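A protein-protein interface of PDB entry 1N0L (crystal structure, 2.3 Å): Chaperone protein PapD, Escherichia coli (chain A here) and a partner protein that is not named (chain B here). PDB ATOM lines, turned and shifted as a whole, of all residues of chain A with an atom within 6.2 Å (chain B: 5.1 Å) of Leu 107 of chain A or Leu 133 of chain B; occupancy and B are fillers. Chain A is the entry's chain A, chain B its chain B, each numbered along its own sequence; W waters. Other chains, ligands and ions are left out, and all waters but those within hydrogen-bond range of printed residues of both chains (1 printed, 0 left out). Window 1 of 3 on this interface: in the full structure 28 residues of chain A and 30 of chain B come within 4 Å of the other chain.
The backbone carbonyl oxygen of Ala 106 of chain A lies within hydrogen-bond range of the backbone NH of Leu 133 of chain B, 2.6 Å away. The backbone NH (N) of Gln 108 of chain A lies within hydrogen-bond range of the backbone carbonyl oxygen (O) of Leu 133 of chain B, at 2.8 Å. NH1 of Arg 91 of chain A is in hydrogen-bond range of OG1 of Thr 132 of chain B (2.8 Å). The backbone NH (N) of Ala 106 of chain A sits at hydrogen-bond distance from the backbone carbonyl oxygen (O) of Ala 131 of chain B, 2.9 Å away. The backbone carbonyl oxygen of Gln 108 of chain A sits at hydrogen-bond distance from the backbone NH of Ala 135 of chain B (2.8 Å).
The backbone NH of Glu 92 of chain A is in hydrogen-bond range of the backbone carbonyl oxygen of Leu 107 of chain A (2.9 Å). The backbone carbonyl oxygen (O) of Thr 47 of chain B is in hydrogen-bond range of the backbone NH (N) of Val 134 of chain B, 2.6 Å away. The backbone NH (N) of Thr 109 of chain A is in hydrogen-bond range of the backbone carbonyl oxygen (O) of Leu 90 of chain A (2.7 Å).
Ala 131 of chain B touches Ile 105 of chain A. CA of Thr 132 of chain B touches O of Ala 106 of chain A, at 3.4 Å. Leu 107 of chain A touches Cys 4 of chain B (CD2 to O, 3.8 Å). Leu 107 of chain A touches Val 6 of chain B. Leu 133 of chain B touches Leu 107 of chain A. Gln 108 of chain A touches Thr 132 of chain B (CB to CG2, 3.4 Å). Val 134 of chain B touches Gln 108 of chain A. O of Ala 135 of chain B touches CA of Thr 109 of chain A (3.6 Å).
Leu 107 of chain A touches just these residues of chain B: Cys 4 (3.8 Å), Val 6 (3.9 Å) and Leu 133 (3.5 Å). Printed residues of chain A within 4 Å of Leu 133 of chain B: Ala 106 (2.6 Å), Leu 107 (3.5 Å) and Gln 108 (2.8 Å). Printed residues of chain A within 4 Å of Ala 135 of chain B: Gln 108 and Thr 109. Printed residues of chain B within 4 Å of Ala 106 of chain A: Ala 131, Thr 132 and Leu 133. Of the printed residues of chain A, Ala 131 of chain B touches Ile 105 (3.4 Å) and Ala 106 (2.9 Å). Printed residues of chain B within 4 Å of Arg 91 of chain A: Thr 132. Printed residues of chain B within 4 Å of Gln 108 of chain A: Thr 132 (3.4 Å), Leu 133 (2.8 Å), Val 134 (3.5 Å) and Ala 135 (2.8 Å). Leu 90 of chain A touches none of the printed residues of chain B. Val 46 of chain B touches none of the printed residues of chain A.
Of the 13 printed residues of chain B, 7 touch a printed residue of chain A. Hydrophobic or aromatic side chains of chain B within 4 Å of the printed part of chain A: Val 6, Ala 131, Leu 133, Val 134 and Ala 135. Among the printed residues, 13 pairs touch across the chains. Among the printed residues, no Asp or Glu carboxylate lies within 4 Å of a Lys or Arg side-chain nitrogen of the other chain.
Water W1 lies within hydrogen-bond range of OG1 of Thr 109 of chain A (2.6 Å) and O of Cys 4 of chain B (2.8 Å).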
ATOM      1  N   VAL A   2       7.090  -9.198  -3.468  1.00  0.00           N
ATOM      2  CA  VAL A   2       7.738  -7.904  -3.672  1.00  0.00           C
ATOM      3  C   VAL A   2       7.692  -7.068  -2.395  1.00  0.00           C
ATOM      4  O   VAL A   2       6.620  -6.831  -1.854  1.00  0.00           O
ATOM      5  CB  VAL A   2       7.031  -7.112  -4.786  1.00  0.00           C
ATOM      6  CG1 VAL A   2       7.695  -5.753  -4.967  1.00  0.00           C
ATOM      7  CG2 VAL A   2       7.059  -7.904  -6.073  1.00  0.00           C
ATOM      8  N   LEU A  90       3.416   0.815  -5.250  1.00  0.00           N
ATOM      9  CA  LEU A  90       4.197  -0.323  -5.723  1.00  0.00           C
ATOM     10  C   LEU A  90       3.270  -1.532  -5.759  1.00  0.00           C
ATOM     11  O   LEU A  90       2.812  -2.014  -4.718  1.00  0.00           O
ATOM     12  CB  LEU A  90       5.371  -0.612  -4.794  1.00  0.00           C
ATOM     13  CG  LEU A  90       6.327  -1.698  -5.306  1.00  0.00           C
ATOM     14  CD1 LEU A  90       6.931  -1.242  -6.631  1.00  0.00           C
ATOM     15  CD2 LEU A  90       7.421  -1.965  -4.277  1.00  0.00           C
ATOM     16  N   ARG A  91       2.978  -2.005  -6.962  1.00  0.00           N
ATOM     17  CA  ARG A  91       2.098  -3.145  -7.124  1.00  0.00           C
ATOM     18  C   ARG A  91       2.858  -4.327  -7.714  1.00  0.00           C
ATOM     19  O   ARG A  91       3.635  -4.184  -8.662  1.00  0.00           O
ATOM     20  CB  ARG A  91       0.924  -2.768  -8.024  1.00  0.00           C
ATOM     21  CG  ARG A  91      -0.125  -3.849  -8.173  1.00  0.00           C
ATOM     22  CD  ARG A  91      -1.333  -3.312  -8.917  1.00  0.00           C
ATOM     23  NE  ARG A  91      -2.380  -4.319  -9.059  1.00  0.00           N
ATOM     24  CZ  ARG A  91      -2.363  -5.296  -9.960  1.00  0.00           C
ATOM     25  NH1 ARG A  91      -3.361  -6.168 -10.015  1.00  0.00           N
ATOM     26  NH2 ARG A  91      -1.355  -5.398 -10.815  1.00  0.00           N
ATOM     27  N   GLU A  92       2.649  -5.499  -7.134  1.00  0.00           N
ATOM     28  CA  GLU A  92       3.333  -6.674  -7.630  1.00  0.00           C
ATOM     29  C   GLU A  92       2.478  -7.442  -8.619  1.00  0.00           C
ATOM     30  O   GLU A  92       1.255  -7.505  -8.487  1.00  0.00           O
ATOM     31  CB  GLU A  92       3.746  -7.593  -6.469  1.00  0.00           C
ATOM     32  CG  GLU A  92       2.684  -7.795  -5.406  1.00  0.00           C
ATOM     33  CD  GLU A  92       3.033  -8.884  -4.404  1.00  0.00           C
ATOM     34  OE1 GLU A  92       4.195  -8.958  -3.950  1.00  0.00           O
ATOM     35  OE2 GLU A  92       2.130  -9.664  -4.057  1.00  0.00           O
ATOM     36  N   ILE A  93       3.124  -7.982  -9.642  1.00  0.00           N
ATOM     37  CA  ILE A  93       2.437  -8.806 -10.627  1.00  0.00           C
ATOM     38  C   ILE A  93       3.067 -10.182 -10.469  1.00  0.00           C
ATOM     39  O   ILE A  93       4.162 -10.431 -10.972  1.00  0.00           O
ATOM     40  CB  ILE A  93       2.661  -8.330 -12.074  1.00  0.00           C
ATOM     41  CG1 ILE A  93       2.064  -6.938 -12.269  1.00  0.00           C
ATOM     42  CG2 ILE A  93       2.017  -9.318 -13.041  1.00  0.00           C
ATOM     43  CD1 ILE A  93       2.183  -6.421 -13.682  1.00  0.00           C
ATOM     44  N   PRO A  94       2.396 -11.080  -9.736  1.00  0.00           N
ATOM     45  CA  PRO A  94       2.884 -12.441  -9.501  1.00  0.00           C
ATOM     46  C   PRO A  94       2.873 -13.309 -10.756  1.00  0.00           C
ATOM     47  O   PRO A  94       1.994 -13.175 -11.611  1.00  0.00           O
ATOM     48  CB  PRO A  94       1.937 -12.961  -8.423  1.00  0.00           C
ATOM     49  CG  PRO A  94       0.668 -12.272  -8.749  1.00  0.00           C
ATOM     50  CD  PRO A  94       1.113 -10.862  -9.050  1.00  0.00           C
ATOM     51  N   ILE A 105      -4.044 -13.133  -5.758  1.00  0.00           N
ATOM     52  CA  ILE A 105      -4.053 -11.982  -4.860  1.00  0.00           C
ATOM     53  C   ILE A 105      -2.726 -11.254  -5.040  1.00  0.00           C
ATOM     54  O   ILE A 105      -1.664 -11.835  -4.837  1.00  0.00           O
ATOM     55  CB  ILE A 105      -4.172 -12.394  -3.380  1.00  0.00           C
ATOM     56  CG1 ILE A 105      -5.583 -12.896  -3.078  1.00  0.00           C
ATOM     57  CG2 ILE A 105      -3.842 -11.206  -2.492  1.00  0.00           C
ATOM     58  CD1 ILE A 105      -6.667 -11.868  -3.326  1.00  0.00           C
ATOM     59  N   ALA A 106      -2.794  -9.992  -5.449  1.00  0.00           N
ATOM     60  CA  ALA A 106      -1.597  -9.183  -5.642  1.00  0.00           C
ATOM     61  C   ALA A 106      -1.550  -8.067  -4.598  1.00  0.00           C
ATOM     62  O   ALA A 106      -2.581  -7.524  -4.199  1.00  0.00           O
ATOM     63  CB  ALA A 106      -1.575  -8.586  -7.047  1.00  0.00           C
ATOM     64  N   LEU A 107      -0.345  -7.728  -4.159  1.00  0.00           N
ATOM     65  CA  LEU A 107      -0.177  -6.687  -3.166  1.00  0.00           C
ATOM     66  C   LEU A 107       0.185  -5.357  -3.795  1.00  0.00           C
ATOM     67  O   LEU A 107       1.046  -5.268  -4.677  1.00  0.00           O
ATOM     68  CB  LEU A 107       0.921  -7.053  -2.157  1.00  0.00           C
ATOM     69  CG  LEU A 107       1.311  -5.935  -1.170  1.00  0.00           C
ATOM     70  CD1 LEU A 107       0.165  -5.673  -0.197  1.00  0.00           C
ATOM     71  CD2 LEU A 107       2.582  -6.335  -0.401  1.00  0.00           C
ATOM     72  N   GLN A 108      -0.494  -4.323  -3.327  1.00  0.00           N
ATOM     73  CA  GLN A 108      -0.214  -2.979  -3.773  1.00  0.00           C
ATOM     74  C   GLN A 108       0.098  -2.178  -2.521  1.00  0.00           C
ATOM     75  O   GLN A 108      -0.728  -2.073  -1.623  1.00  0.00           O
ATOM     76  CB  GLN A 108      -1.407  -2.360  -4.484  1.00  0.00           C
ATOM     77  CG  GLN A 108      -1.050  -1.030  -5.135  1.00  0.00           C
ATOM     78  CD  GLN A 108      -2.267  -0.236  -5.549  1.00  0.00           C
ATOM     79  OE1 GLN A 108      -3.210  -0.780  -6.127  1.00  0.00           O
ATOM     80  NE2 GLN A 108      -2.252   1.063  -5.263  1.00  0.00           N
ATOM     81  N   THR A 109       1.304  -1.641  -2.462  1.00  0.00           N
ATOM     82  CA  THR A 109       1.737  -0.836  -1.342  1.00  0.00           C
ATOM     83  C   THR A 109       1.648   0.646  -1.725  1.00  0.00           C
ATOM     84  O   THR A 109       2.206   1.065  -2.740  1.00  0.00           O
ATOM     85  CB  THR A 109       3.190  -1.179  -0.961  1.00  0.00           C
ATOM     86  OG1 THR A 109       3.229  -2.477  -0.342  1.00  0.00           O
ATOM     87  CG2 THR A 109       3.754  -0.133  -0.004  1.00  0.00           C
ATOM     88  N   CYS B   4       4.780  -4.076   4.855  1.00  0.00           N
ATOM     89  CA  CYS B   4       4.372  -5.459   5.005  1.00  0.00           C
ATOM     90  C   CYS B   4       4.639  -6.155   3.683  1.00  0.00           C
ATOM     91  O   CYS B   4       4.697  -5.516   2.630  1.00  0.00           O
ATOM     92  CB  CYS B   4       2.879  -5.581   5.263  1.00  0.00           C
ATOM     93  SG  CYS B   4       2.137  -4.736   6.689  1.00  0.00           S
ATOM     94  N   THR B   5       4.786  -7.469   3.737  1.00  0.00           N
ATOM     95  CA  THR B   5       4.995  -8.251   2.529  1.00  0.00           C
ATOM     96  C   THR B   5       3.874  -9.272   2.517  1.00  0.00           C
ATOM     97  O   THR B   5       3.339  -9.616   3.561  1.00  0.00           O
ATOM     98  CB  THR B   5       6.346  -8.997   2.547  1.00  0.00           C
ATOM     99  OG1 THR B   5       6.385  -9.890   3.666  1.00  0.00           O
ATOM    100  CG2 THR B   5       7.499  -8.014   2.657  1.00  0.00           C
ATOM    101  N   VAL B   6       3.495  -9.732   1.335  1.00  0.00           N
ATOM    102  CA  VAL B   6       2.454 -10.743   1.218  1.00  0.00           C
ATOM    103  C   VAL B   6       3.038 -11.871   0.383  1.00  0.00           C
ATOM    104  O   VAL B   6       3.525 -11.645  -0.728  1.00  0.00           O
ATOM    105  CB  VAL B   6       1.182 -10.197   0.510  1.00  0.00           C
ATOM    106  CG1 VAL B   6       0.262 -11.348   0.133  1.00  0.00           C
ATOM    107  CG2 VAL B   6       0.436  -9.239   1.431  1.00  0.00           C
ATOM    108  N   VAL B  33      -4.607 -15.029   3.846  1.00  0.00           N
ATOM    109  CA  VAL B  33      -3.553 -14.166   3.351  1.00  0.00           C
ATOM    110  C   VAL B  33      -2.773 -13.787   4.598  1.00  0.00           C
ATOM    111  O   VAL B  33      -3.343 -13.260   5.549  1.00  0.00           O
ATOM    112  CB  VAL B  33      -4.113 -12.889   2.685  1.00  0.00           C
ATOM    113  CG1 VAL B  33      -5.093 -12.198   3.611  1.00  0.00           C
ATOM    114  CG2 VAL B  33      -2.971 -11.950   2.339  1.00  0.00           C
ATOM    115  N   MET B  35       0.264 -11.553   6.086  1.00  0.00           N
ATOM    116  CA  MET B  35       1.164 -10.439   5.848  1.00  0.00           C
ATOM    117  C   MET B  35       2.224 -10.379   6.932  1.00  0.00           C
ATOM    118  O   MET B  35       1.918 -10.538   8.107  1.00  0.00           O
ATOM    119  CB  MET B  35       0.374  -9.135   5.845  1.00  0.00           C
ATOM    120  CG  MET B  35      -1.063  -9.296   5.403  1.00  0.00           C
ATOM    121  SD  MET B  35      -1.905  -7.613   5.040  1.00  0.00           S
ATOM    122  CE  MET B  35      -2.672  -7.252   6.770  1.00  0.00           C
ATOM    123  N   VAL B  46      -7.125  -2.530   5.078  1.00  0.00           N
ATOM    124  CA  VAL B  46      -6.727  -2.764   3.693  1.00  0.00           C
ATOM    125  C   VAL B  46      -7.903  -2.634   2.738  1.00  0.00           C
ATOM    126  O   VAL B  46      -9.062  -2.624   3.164  1.00  0.00           O
ATOM    127  CB  VAL B  46      -6.116  -4.162   3.521  1.00  0.00           C
ATOM    128  CG1 VAL B  46      -4.759  -4.227   4.228  1.00  0.00           C
ATOM    129  CG2 VAL B  46      -7.064  -5.202   4.087  1.00  0.00           C
ATOM    130  N   THR B  47      -7.596  -2.533   1.446  1.00  0.00           N
ATOM    131  CA  THR B  47      -8.623  -2.395   0.420  1.00  0.00           C
ATOM    132  C   THR B  47      -8.432  -3.438  -0.667  1.00  0.00           C
ATOM    133  O   THR B  47      -7.316  -3.682  -1.112  1.00  0.00           O
ATOM    134  CB  THR B  47      -8.561  -1.010  -0.283  1.00  0.00           C
ATOM    135  OG1 THR B  47      -8.506   0.033   0.692  1.00  0.00           O
ATOM    136  CG2 THR B  47      -9.790  -0.808  -1.171  1.00  0.00           C
ATOM    137  N   ILE B  48      -9.519  -4.059  -1.099  1.00  0.00           N
ATOM    138  CA  ILE B  48      -9.416  -5.030  -2.170  1.00  0.00           C
ATOM    139  C   ILE B  48     -10.098  -4.445  -3.387  1.00  0.00           C
ATOM    140  O   ILE B  48     -11.273  -4.087  -3.342  1.00  0.00           O
ATOM    141  CB  ILE B  48     -10.105  -6.359  -1.824  1.00  0.00           C
ATOM    142  CG1 ILE B  48      -9.435  -6.992  -0.605  1.00  0.00           C
ATOM    143  CG2 ILE B  48     -10.006  -7.313  -3.002  1.00  0.00           C
ATOM    144  CD1 ILE B  48     -10.209  -8.145  -0.028  1.00  0.00           C
ATOM    145  N   ALA B 131      -6.930 -10.016  -8.019  1.00  0.00           N
ATOM    146  CA  ALA B 131      -7.511  -9.070  -7.084  1.00  0.00           C
ATOM    147  C   ALA B 131      -6.383  -8.373  -6.347  1.00  0.00           C
ATOM    148  O   ALA B 131      -5.500  -9.023  -5.784  1.00  0.00           O
ATOM    149  CB  ALA B 131      -8.405  -9.793  -6.104  1.00  0.00           C
ATOM    150  N   THR B 132      -6.410  -7.045  -6.353  1.00  0.00           N
ATOM    151  CA  THR B 132      -5.374  -6.276  -5.689  1.00  0.00           C
ATOM    152  C   THR B 132      -5.697  -5.972  -4.241  1.00  0.00           C
ATOM    153  O   THR B 132      -6.758  -5.433  -3.910  1.00  0.00           O
ATOM    154  CB  THR B 132      -5.109  -4.967  -6.416  1.00  0.00           C
ATOM    155  OG1 THR B 132      -4.708  -5.254  -7.759  1.00  0.00           O
ATOM    156  CG2 THR B 132      -4.000  -4.183  -5.719  1.00  0.00           C
ATOM    157  N   LEU B 133      -4.760  -6.350  -3.381  1.00  0.00           N
ATOM    158  CA  LEU B 133      -4.863  -6.122  -1.952  1.00  0.00           C
ATOM    159  C   LEU B 133      -4.072  -4.846  -1.739  1.00  0.00           C
ATOM    160  O   LEU B 133      -2.840  -4.850  -1.846  1.00  0.00           O
ATOM    161  CB  LEU B 133      -4.217  -7.269  -1.190  1.00  0.00           C
ATOM    162  CG  LEU B 133      -4.012  -7.062   0.306  1.00  0.00           C
ATOM    163  CD1 LEU B 133      -5.358  -6.962   1.027  1.00  0.00           C
ATOM    164  CD2 LEU B 133      -3.185  -8.230   0.844  1.00  0.00           C
ATOM    165  N   VAL B 134      -4.779  -3.758  -1.458  1.00  0.00           N
ATOM    166  CA  VAL B 134      -4.137  -2.467  -1.258  1.00  0.00           C
ATOM    167  C   VAL B 134      -3.804  -2.146   0.188  1.00  0.00           C
ATOM    168  O   VAL B 134      -4.701  -2.036   1.023  1.00  0.00           O
ATOM    169  CB  VAL B 134      -5.009  -1.307  -1.801  1.00  0.00           C
ATOM    170  CG1 VAL B 134      -4.237   0.032  -1.688  1.00  0.00           C
ATOM    171  CG2 VAL B 134      -5.393  -1.575  -3.243  1.00  0.00           C
ATOM    172  N   ALA B 135      -2.514  -1.994   0.479  1.00  0.00           N
ATOM    173  CA  ALA B 135      -2.086  -1.634   1.827  1.00  0.00           C
ATOM    174  C   ALA B 135      -1.623  -0.182   1.760  1.00  0.00           C
ATOM    175  O   ALA B 135      -0.557   0.121   1.212  1.00  0.00           O
ATOM    176  CB  ALA B 135      -0.945  -2.540   2.310  1.00  0.00           C
HETATM  177  O   HOH W   1       2.803  -3.641   1.893  1.00  0.00           O
